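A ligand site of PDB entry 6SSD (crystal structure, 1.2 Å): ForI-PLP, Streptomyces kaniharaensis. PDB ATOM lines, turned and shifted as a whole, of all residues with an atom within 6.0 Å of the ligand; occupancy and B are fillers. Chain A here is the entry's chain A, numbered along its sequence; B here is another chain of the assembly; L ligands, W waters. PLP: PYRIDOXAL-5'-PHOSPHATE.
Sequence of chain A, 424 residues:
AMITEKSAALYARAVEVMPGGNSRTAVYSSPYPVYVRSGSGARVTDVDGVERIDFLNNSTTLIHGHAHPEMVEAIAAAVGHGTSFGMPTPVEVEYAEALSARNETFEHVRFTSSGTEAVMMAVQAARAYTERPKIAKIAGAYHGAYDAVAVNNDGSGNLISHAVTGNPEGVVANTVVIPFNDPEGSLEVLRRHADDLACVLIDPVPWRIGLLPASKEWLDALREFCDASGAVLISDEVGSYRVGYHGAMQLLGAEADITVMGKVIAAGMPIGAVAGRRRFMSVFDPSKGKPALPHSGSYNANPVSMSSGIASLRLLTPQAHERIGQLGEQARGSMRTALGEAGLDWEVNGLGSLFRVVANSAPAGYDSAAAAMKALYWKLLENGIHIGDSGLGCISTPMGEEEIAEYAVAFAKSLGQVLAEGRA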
ATOM      1  N   SER A  59       2.042  18.232 -27.292  1.00  0.00           N
ATOM      2  CA  SER A  59       2.817  18.229 -26.061  1.00  0.00           C
ATOM      3  C   SER A  59       3.940  17.202 -26.077  1.00  0.00           C
ATOM      4  O   SER A  59       4.179  16.540 -25.080  1.00  0.00           O
ATOM      5  CB  SER A  59       1.904  18.014 -24.846  1.00  0.00           C
ATOM      6  OG  SER A  59       1.189  19.208 -24.664  1.00  0.00           O
ATOM      7  N   SER A 113      -3.668   3.349 -20.088  1.00  0.00           N
ATOM      8  CA  SER A 113      -4.225   4.220 -21.131  1.00  0.00           C
ATOM      9  C   SER A 113      -3.698   5.633 -21.154  1.00  0.00           C
ATOM     10  O   SER A 113      -4.057   6.418 -22.029  1.00  0.00           O
ATOM     11  CB  SER A 113      -5.745   4.195 -21.088  1.00  0.00           C
ATOM     12  OG  SER A 113      -6.226   2.951 -21.596  1.00  0.00           O
ATOM     13  N   SER A 114      -2.811   5.968 -20.209  1.00  0.00           N
ATOM     14  CA  SER A 114      -2.228   7.291 -20.151  1.00  0.00           C
ATOM     15  C   SER A 114      -0.986   7.286 -19.279  1.00  0.00           C
ATOM     16  O   SER A 114      -0.801   6.371 -18.435  1.00  0.00           O
ATOM     17  CB  SER A 114      -3.215   8.310 -19.593  1.00  0.00           C
ATOM     18  OG  SER A 114      -3.441   8.018 -18.214  1.00  0.00           O
ATOM     19  N   GLY A 115      -0.138   8.287 -19.475  1.00  0.00           N
ATOM     20  CA  GLY A 115       0.979   8.498 -18.569  1.00  0.00           C
ATOM     21  C   GLY A 115       0.528   8.795 -17.165  1.00  0.00           C
ATOM     22  O   GLY A 115       1.173   8.404 -16.186  1.00  0.00           O
ATOM     23  N   THR A 116      -0.597   9.515 -17.040  1.00  0.00           N
ATOM     24  CA  THR A 116      -1.154   9.828 -15.722  1.00  0.00           C
ATOM     25  C   THR A 116      -1.449   8.542 -14.937  1.00  0.00           C
ATOM     26  O   THR A 116      -1.095   8.466 -13.749  1.00  0.00           O
ATOM     27  CB  THR A 116      -2.407  10.692 -15.931  1.00  0.00           C
ATOM     28  OG1 THR A 116      -1.990  11.968 -16.453  1.00  0.00           O
ATOM     29  CG2 THR A 116      -3.215  10.896 -14.676  1.00  0.00           C
ATOM     30  N   GLU A 117      -2.119   7.611 -15.586  1.00  0.00           N
ATOM     31  CA  GLU A 117      -2.383   6.316 -14.962  1.00  0.00           C
ATOM     32  C   GLU A 117      -1.098   5.561 -14.651  1.00  0.00           C
ATOM     33  O   GLU A 117      -0.995   4.905 -13.620  1.00  0.00           O
ATOM     34  CB  GLU A 117      -3.236   5.421 -15.858  1.00  0.00           C
ATOM     35  CG  GLU A 117      -4.696   5.733 -15.966  1.00  0.00           C
ATOM     36  CD  GLU A 117      -5.499   4.698 -16.800  1.00  0.00           C
ATOM     37  OE1 GLU A 117      -6.727   4.771 -16.733  1.00  0.00           O
ATOM     38  OE2 GLU A 117      -4.877   3.829 -17.489  1.00  0.00           O
ATOM     39  N   VAL A 119       1.955   6.719 -14.040  1.00  0.00           N
ATOM     40  CA  VAL A 119       2.627   7.257 -12.855  1.00  0.00           C
ATOM     41  C   VAL A 119       1.931   6.789 -11.583  1.00  0.00           C
ATOM     42  O   VAL A 119       2.581   6.386 -10.602  1.00  0.00           O
ATOM     43  CB  VAL A 119       2.676   8.799 -12.900  1.00  0.00           C
ATOM     44  CG1 VAL A 119       3.097   9.372 -11.535  1.00  0.00           C
ATOM     45  CG2 VAL A 119       3.548   9.342 -13.987  1.00  0.00           C
ATOM     46  N   TYR A 142       6.051  18.184 -12.987  1.00  0.00           N
ATOM     47  CA  TYR A 142       4.695  17.688 -13.286  1.00  0.00           C
ATOM     48  C   TYR A 142       4.690  16.233 -13.635  1.00  0.00           C
ATOM     49  O   TYR A 142       5.542  15.766 -14.410  1.00  0.00           O
ATOM     50  CB  TYR A 142       4.125  18.427 -14.491  1.00  0.00           C
ATOM     51  CG  TYR A 142       2.845  17.863 -15.125  1.00  0.00           C
ATOM     52  CD1 TYR A 142       1.593  18.203 -14.632  1.00  0.00           C
ATOM     53  CD2 TYR A 142       2.898  17.036 -16.244  1.00  0.00           C
ATOM     54  CE1 TYR A 142       0.426  17.753 -15.246  1.00  0.00           C
ATOM     55  CE2 TYR A 142       1.758  16.573 -16.852  1.00  0.00           C
ATOM     56  CZ  TYR A 142       0.529  16.947 -16.346  1.00  0.00           C
ATOM     57  OH  TYR A 142      -0.653  16.526 -16.920  1.00  0.00           O
ATOM     58  N   HIS A 143       3.670  15.526 -13.139  1.00  0.00           N
ATOM     59  CA  HIS A 143       3.489  14.102 -13.381  1.00  0.00           C
ATOM     60  C   HIS A 143       2.048  13.708 -13.652  1.00  0.00           C
ATOM     61  O   HIS A 143       1.730  12.539 -13.533  1.00  0.00           O
ATOM     62  CB  HIS A 143       4.035  13.269 -12.193  1.00  0.00           C
ATOM     63  CG  HIS A 143       5.464  13.545 -11.858  1.00  0.00           C
ATOM     64  ND1 HIS A 143       6.522  12.951 -12.510  1.00  0.00           N
ATOM     65  CD2 HIS A 143       6.014  14.328 -10.889  1.00  0.00           C
ATOM     66  CE1 HIS A 143       7.653  13.400 -11.985  1.00  0.00           C
ATOM     67  NE2 HIS A 143       7.380  14.241 -10.997  1.00  0.00           N
ATOM     68  N   GLY A 144       1.208  14.681 -13.982  1.00  0.00           N
ATOM     69  CA  GLY A 144      -0.211  14.442 -14.180  1.00  0.00           C
ATOM     70  C   GLY A 144      -1.035  14.692 -12.924  1.00  0.00           C
ATOM     71  O   GLY A 144      -0.541  15.122 -11.881  1.00  0.00           O
ATOM     72  N   ASP A 203      11.846  13.087 -12.744  1.00  0.00           N
ATOM     73  CA  ASP A 203      11.884  13.167 -14.218  1.00  0.00           C
ATOM     74  C   ASP A 203      13.309  13.589 -14.499  1.00  0.00           C
ATOM     75  O   ASP A 203      13.748  14.600 -13.969  1.00  0.00           O
ATOM     76  CB  ASP A 203      10.855  14.208 -14.706  1.00  0.00           C
ATOM     77  CG  ASP A 203      10.860  14.433 -16.195  1.00  0.00           C
ATOM     78  OD1 ASP A 203      11.830  14.068 -16.884  1.00  0.00           O
ATOM     79  OD2 ASP A 203       9.826  15.010 -16.667  1.00  0.00           O
ATOM     80  N   TRP A 207      10.578  19.590 -18.021  1.00  0.00           N
ATOM     81  CA  TRP A 207      10.541  20.833 -18.763  1.00  0.00           C
ATOM     82  C   TRP A 207      10.054  22.012 -17.954  1.00  0.00           C
ATOM     83  O   TRP A 207      10.480  23.141 -18.221  1.00  0.00           O
ATOM     84  CB  TRP A 207       9.770  20.699 -20.065  1.00  0.00           C
ATOM     85  CG  TRP A 207       8.296  20.678 -20.064  1.00  0.00           C
ATOM     86  CD1 TRP A 207       7.518  19.609 -20.304  1.00  0.00           C
ATOM     87  CD2 TRP A 207       7.403  21.806 -19.997  1.00  0.00           C
ATOM     88  NE1 TRP A 207       6.214  19.966 -20.342  1.00  0.00           N
ATOM     89  CE2 TRP A 207       6.109  21.321 -20.159  1.00  0.00           C
ATOM     90  CE3 TRP A 207       7.592  23.177 -19.883  1.00  0.00           C
ATOM     91  CZ2 TRP A 207       4.995  22.166 -20.156  1.00  0.00           C
ATOM     92  CZ3 TRP A 207       6.514  24.004 -19.896  1.00  0.00           C
ATOM     93  CH2 TRP A 207       5.229  23.513 -20.015  1.00  0.00           C
ATOM     94  N   ARG A 208       9.157  21.787 -16.984  1.00  0.00           N
ATOM     95  CA  ARG A 208       8.524  22.913 -16.330  1.00  0.00           C
ATOM     96  C   ARG A 208       9.470  23.720 -15.443  1.00  0.00           C
ATOM     97  O   ARG A 208       9.178  24.877 -15.127  1.00  0.00           O
ATOM     98  CB  ARG A 208       7.331  22.471 -15.530  1.00  0.00           C
ATOM     99  CG  ARG A 208       6.180  22.170 -16.445  1.00  0.00           C
ATOM    100  CD  ARG A 208       5.082  21.466 -15.762  1.00  0.00           C
ATOM    101  NE  ARG A 208       4.081  20.985 -16.735  1.00  0.00           N
ATOM    102  CZ  ARG A 208       4.191  19.920 -17.567  1.00  0.00           C
ATOM    103  NH1 ARG A 208       5.313  19.097 -17.545  1.00  0.00           N
ATOM    104  NH2 ARG A 208       3.167  19.641 -18.442  1.00  0.00           N
ATOM    105  N   ASP A 236      10.176   9.029 -14.181  1.00  0.00           N
ATOM    106  CA  ASP A 236       9.032   9.369 -15.041  1.00  0.00           C
ATOM    107  C   ASP A 236       9.591   9.994 -16.289  1.00  0.00           C
ATOM    108  O   ASP A 236       9.978  11.162 -16.321  1.00  0.00           O
ATOM    109  CB  ASP A 236       8.085  10.316 -14.331  1.00  0.00           C
ATOM    110  CG  ASP A 236       6.903  10.703 -15.195  1.00  0.00           C
ATOM    111  OD1 ASP A 236       6.841  10.288 -16.380  1.00  0.00           O
ATOM    112  OD2 ASP A 236       6.020  11.445 -14.666  1.00  0.00           O
ATOM    113  N   GLU A 237       9.605   9.181 -17.356  1.00  0.00           N
ATOM    114  CA  GLU A 237      10.096   9.544 -18.667  1.00  0.00           C
ATOM    115  C   GLU A 237       8.955   9.663 -19.656  1.00  0.00           C
ATOM    116  O   GLU A 237       9.185   9.589 -20.880  1.00  0.00           O
ATOM    117  CB  GLU A 237      11.153   8.516 -19.145  1.00  0.00           C
ATOM    118  CG  GLU A 237      12.331   8.491 -18.183  1.00  0.00           C
ATOM    119  CD  GLU A 237      13.530   7.720 -18.618  1.00  0.00           C
ATOM    120  OE1 GLU A 237      13.636   7.405 -19.816  1.00  0.00           O
ATOM    121  OE2 GLU A 237      14.401   7.462 -17.743  1.00  0.00           O
ATOM    122  N   VAL A 238       7.730   9.919 -19.181  1.00  0.00           N
ATOM    123  CA  VAL A 238       6.600  10.054 -20.137  1.00  0.00           C
ATOM    124  C   VAL A 238       6.937  11.133 -21.173  1.00  0.00           C
ATOM    125  O   VAL A 238       6.660  10.936 -22.350  1.00  0.00           O
ATOM    126  CB  VAL A 238       5.272  10.299 -19.397  1.00  0.00           C
ATOM    127  CG1 VAL A 238       4.185  10.567 -20.395  1.00  0.00           C
ATOM    128  CG2 VAL A 238       4.907   9.085 -18.559  1.00  0.00           C
ATOM    129  N   GLY A 239       7.491  12.258 -20.739  1.00  0.00           N
ATOM    130  CA  GLY A 239       7.945  13.306 -21.651  1.00  0.00           C
ATOM    131  C   GLY A 239       9.387  13.252 -22.076  1.00  0.00           C
ATOM    132  O   GLY A 239       9.711  13.620 -23.212  1.00  0.00           O
ATOM    133  N   SER A 240      10.273  12.804 -21.184  1.00  0.00           N
ATOM    134  CA  SER A 240      11.695  12.917 -21.433  1.00  0.00           C
ATOM    135  C   SER A 240      12.340  11.686 -22.048  1.00  0.00           C
ATOM    136  O   SER A 240      13.503  11.758 -22.451  1.00  0.00           O
ATOM    137  CB  SER A 240      12.462  13.319 -20.163  1.00  0.00           C
ATOM    138  OG  SER A 240      12.253  12.395 -19.124  1.00  0.00           O
ATOM    139  N   GLY A 262       5.248   6.949 -21.894  1.00  0.00           N
ATOM    140  CA  GLY A 262       4.035   7.293 -22.581  1.00  0.00           C
ATOM    141  C   GLY A 262       4.372   8.126 -23.813  1.00  0.00           C
ATOM    142  O   GLY A 262       5.465   7.960 -24.376  1.00  0.00           O
ATOM    143  N   LYS A 263       3.444   9.001 -24.174  1.00  0.00           N
ATOM    144  CA  LYS A 263       3.657   9.980 -25.266  1.00  0.00           C
ATOM    145  C   LYS A 263       4.299   9.294 -26.479  1.00  0.00           C
ATOM    146  O   LYS A 263       3.589   8.588 -27.213  1.00  0.00           O
ATOM    147  CB  LYS A 263       4.363  11.235 -24.740  1.00  0.00           C
ATOM    148  CG  LYS A 263       3.441  12.060 -23.817  1.00  0.00           C
ATOM    149  CD  LYS A 263       4.032  13.428 -23.551  1.00  0.00           C
ATOM    150  CE  LYS A 263       3.205  14.359 -22.671  1.00  0.00           C
ATOM    151  NZ  LYS A 263       3.608  14.247 -21.259  1.00  0.00           N
ATOM    152  N   ILE A 271      -1.873   5.798 -24.419  1.00  0.00           N
ATOM    153  CA  ILE A 271      -1.036   4.777 -23.814  1.00  0.00           C
ATOM    154  C   ILE A 271      -0.271   5.356 -22.638  1.00  0.00           C
ATOM    155  O   ILE A 271      -0.041   6.565 -22.552  1.00  0.00           O
ATOM    156  CB  ILE A 271      -0.035   4.196 -24.845  1.00  0.00           C
ATOM    157  CG1 ILE A 271       0.419   2.788 -24.464  1.00  0.00           C
ATOM    158  CG2 ILE A 271       1.153   5.098 -25.081  1.00  0.00           C
ATOM    159  CD1 ILE A 271       1.140   2.074 -25.587  1.00  0.00           C
ATOM    160  N   GLU B 117      -9.703   7.354 -14.739  1.00  0.00           N
ATOM    161  CA  GLU B 117      -9.363   8.773 -14.643  1.00  0.00           C
ATOM    162  C   GLU B 117     -10.584   9.632 -14.343  1.00  0.00           C
ATOM    163  O   GLU B 117     -10.497  10.594 -13.586  1.00  0.00           O
ATOM    164  CB  GLU B 117      -8.742   9.293 -15.937  1.00  0.00           C
ATOM    165  CG  GLU B 117      -7.325   8.912 -16.231  1.00  0.00           C
ATOM    166  CD  GLU B 117      -6.745   9.587 -17.504  1.00  0.00           C
ATOM    167  OE1 GLU B 117      -5.527   9.497 -17.669  1.00  0.00           O
ATOM    168  OE2 GLU B 117      -7.524  10.202 -18.299  1.00  0.00           O
ATOM    169  N   SER B 296      -5.518  18.134 -17.185  1.00  0.00           N
ATOM    170  CA  SER B 296      -5.026  17.979 -18.559  1.00  0.00           C
ATOM    171  C   SER B 296      -4.935  16.460 -18.850  1.00  0.00           C
ATOM    172  O   SER B 296      -5.692  15.690 -18.263  1.00  0.00           O
ATOM    173  CB  SER B 296      -3.748  18.789 -18.768  1.00  0.00           C
ATOM    174  OG  SER B 296      -4.042  20.164 -18.583  1.00  0.00           O
ATOM    175  N   GLY B 297      -4.096  16.092 -19.821  1.00  0.00           N
ATOM    176  CA  GLY B 297      -3.993  14.710 -20.266  1.00  0.00           C
ATOM    177  C   GLY B 297      -3.870  14.679 -21.789  1.00  0.00           C
ATOM    178  O   GLY B 297      -4.691  15.265 -22.509  1.00  0.00           O
ATOM    179  N   SER B 298      -2.844  13.981 -22.268  1.00  0.00           N
ATOM    180  CA  SER B 298      -2.444  14.068 -23.682  1.00  0.00           C
ATOM    181  C   SER B 298      -3.520  13.652 -24.643  1.00  0.00           C
ATOM    182  O   SER B 298      -3.490  14.081 -25.809  1.00  0.00           O
ATOM    183  CB  SER B 298      -1.182  13.220 -23.901  1.00  0.00           C
ATOM    184  OG  SER B 298      -0.082  13.676 -23.165  1.00  0.00           O
ATOM    185  N   TYR B 299      -4.414  12.730 -24.232  1.00  0.00           N
ATOM    186  CA  TYR B 299      -5.420  12.182 -25.121  1.00  0.00           C
ATOM    187  C   TYR B 299      -6.816  12.676 -24.784  1.00  0.00           C
ATOM    188  O   TYR B 299      -7.789  12.202 -25.379  1.00  0.00           O
ATOM    189  CB  TYR B 299      -5.327  10.639 -25.199  1.00  0.00           C
ATOM    190  CG  TYR B 299      -3.904  10.179 -25.242  1.00  0.00           C
ATOM    191  CD1 TYR B 299      -3.137  10.232 -26.393  1.00  0.00           C
ATOM    192  CD2 TYR B 299      -3.274   9.771 -24.063  1.00  0.00           C
ATOM    193  CE1 TYR B 299      -1.799   9.934 -26.404  1.00  0.00           C
ATOM    194  CE2 TYR B 299      -1.924   9.460 -24.037  1.00  0.00           C
ATOM    195  CZ  TYR B 299      -1.185   9.554 -25.199  1.00  0.00           C
ATOM    196  OH  TYR B 299       0.175   9.277 -25.231  1.00  0.00           O
HETATM  197  N1  PLP L   1       4.439  12.658 -16.553  1.00  0.00           N
HETATM  198  C2  PLP L   1       5.174  13.435 -17.319  1.00  0.00           C
HETATM  199  C2A PLP L   1       6.576  13.744 -16.885  1.00  0.00           C
HETATM  200  C3  PLP L   1       4.668  13.837 -18.603  1.00  0.00           C
HETATM  201  O3  PLP L   1       5.465  14.499 -19.436  1.00  0.00           O
HETATM  202  C4  PLP L   1       3.319  13.534 -18.964  1.00  0.00           C
HETATM  203  C4A PLP L   1       2.751  13.765 -20.278  1.00  0.00           C
HETATM  204  C5  PLP L   1       2.531  12.838 -17.954  1.00  0.00           C
HETATM  205  C6  PLP L   1       3.170  12.339 -16.854  1.00  0.00           C
HETATM  206  C5A PLP L   1       1.079  12.540 -18.153  1.00  0.00           C
HETATM  207  O4P PLP L   1       0.861  11.666 -19.257  1.00  0.00           O
HETATM  208  P   PLP L   1      -0.562  11.676 -20.039  1.00  0.00           P
HETATM  209  O1P PLP L   1      -1.616  11.408 -19.008  1.00  0.00           O
HETATM  210  O2P PLP L   1      -0.686  13.049 -20.643  1.00  0.00           O
HETATM  211  O3P PLP L   1      -0.414  10.541 -21.050  1.00  0.00           O
HETATM  212  O   HOH W   1       6.545  16.714 -19.338  1.00  0.00           O
HETATM  213  O   HOH W   2       1.102   9.091 -22.636  1.00  0.00           O
HETATM  214  O   HOH W   3      -0.625  15.516 -19.477  1.00  0.00           O
HETATM  215  O   HOH W   4      -4.430  11.505 -19.196  1.00  0.00           O
HETATM  216  O   HOH W   5       9.248  12.841 -18.428  1.00  0.00           O
HETATM  217  O   HOH W   6       1.951  17.127 -20.321  1.00  0.00           O
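Water W1 lies within hydrogen-bond range of an oxygen (O3) of the ligand, the guanidinium group (NH1) of Arg 208 and the indole nitrogen (NE1) of Trp 207.
Water W2 lies within hydrogen-bond range of O3P of the ligand, OH of Tyr 299 of chain B, O of Ile 271, N of Lys 263 and N of Gly 115.
Water W3 lies within hydrogen-bond range of O2P of the ligand (2.7 Å) and OH of Tyr 142 (2.7 Å).
Water W4 lies within hydrogen-bond range of OE1 of Glu 117 of chain B (2.8 Å) and O1P of the ligand (2.8 Å).
Water W6 bridges the guanidinium group (NH2) of Arg 208 (3.4 Å) and the side-chain amino group (NZ) of Lys 263 (3.5 Å).
The side-chain hydroxyl (OG) of Ser 114 lies within hydrogen-bond range of the side-chain carboxylate (OE1) of Glu 117 of chain B (2.6 Å).
The side-chain carboxylate of Asp 203 sits at hydrogen-bond distance from the side-chain hydroxyl of Ser 240 (2.8 Å).
The side-chain hydroxyl (OG) of Ser 114 sits close to the backbone NH (N) of Thr 116.
The side-chain hydroxyl (OG) of Ser 114 sits at hydrogen-bond distance from the backbone NH (N) of Glu 117 of chain A (3.0 Å).
The backbone NH (N) of Lys 263 is in hydrogen-bond range of the side-chain hydroxyl (OH) of Tyr 299 of chain B, at 3.4 Å.
The side-chain carboxylate (OD1) of Asp 236 lies within hydrogen-bond range of the backbone NH (N) of Val 238 (3.0 Å).
OD2 of Asp 236 sits at hydrogen-bond distance from ND1 of His 143, 2.7 Å away.
The side-chain hydroxyl (OG1) of Thr 116 is in hydrogen-bond range of an oxygen (O1P) of the ligand, 2.6 Å away.
The backbone NH (N) of Gly 115 sits at hydrogen-bond distance from an oxygen (O3P) of the ligand (2.8 Å).
OD2 of Asp 236 sits at hydrogen-bond distance from N1 of the ligand (2.7 Å).
O1P of the ligand lies within hydrogen-bond range of N of Thr 116, at 2.9 Å.
C4A of the ligand is covalently linked to NZ of Lys 263, at 1.4 Å.
The backbone NH (N) of Ser 298 of chain B lies within hydrogen-bond range of an oxygen (O2P) of the ligand (2.9 Å).
O2P of the ligand lies within hydrogen-bond range of OG of Ser 298 of chain B (2.7 Å).
O3 of the ligand is in hydrogen-bond range of N of Gly 239 (3.3 Å).
CB of Ser 114 touches O1P of the ligand (3.5 Å).
Tyr 142 touches the ligand.
His 143 touches the ligand (CA to N1, 3.6 Å).
Asp 203 touches the ligand (OD2 to C2A, 3.5 Å).
Val 238 touches the ligand.
Gly 297 of chain B touches the ligand.
Tyr 299 of chain B touches the ligand.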
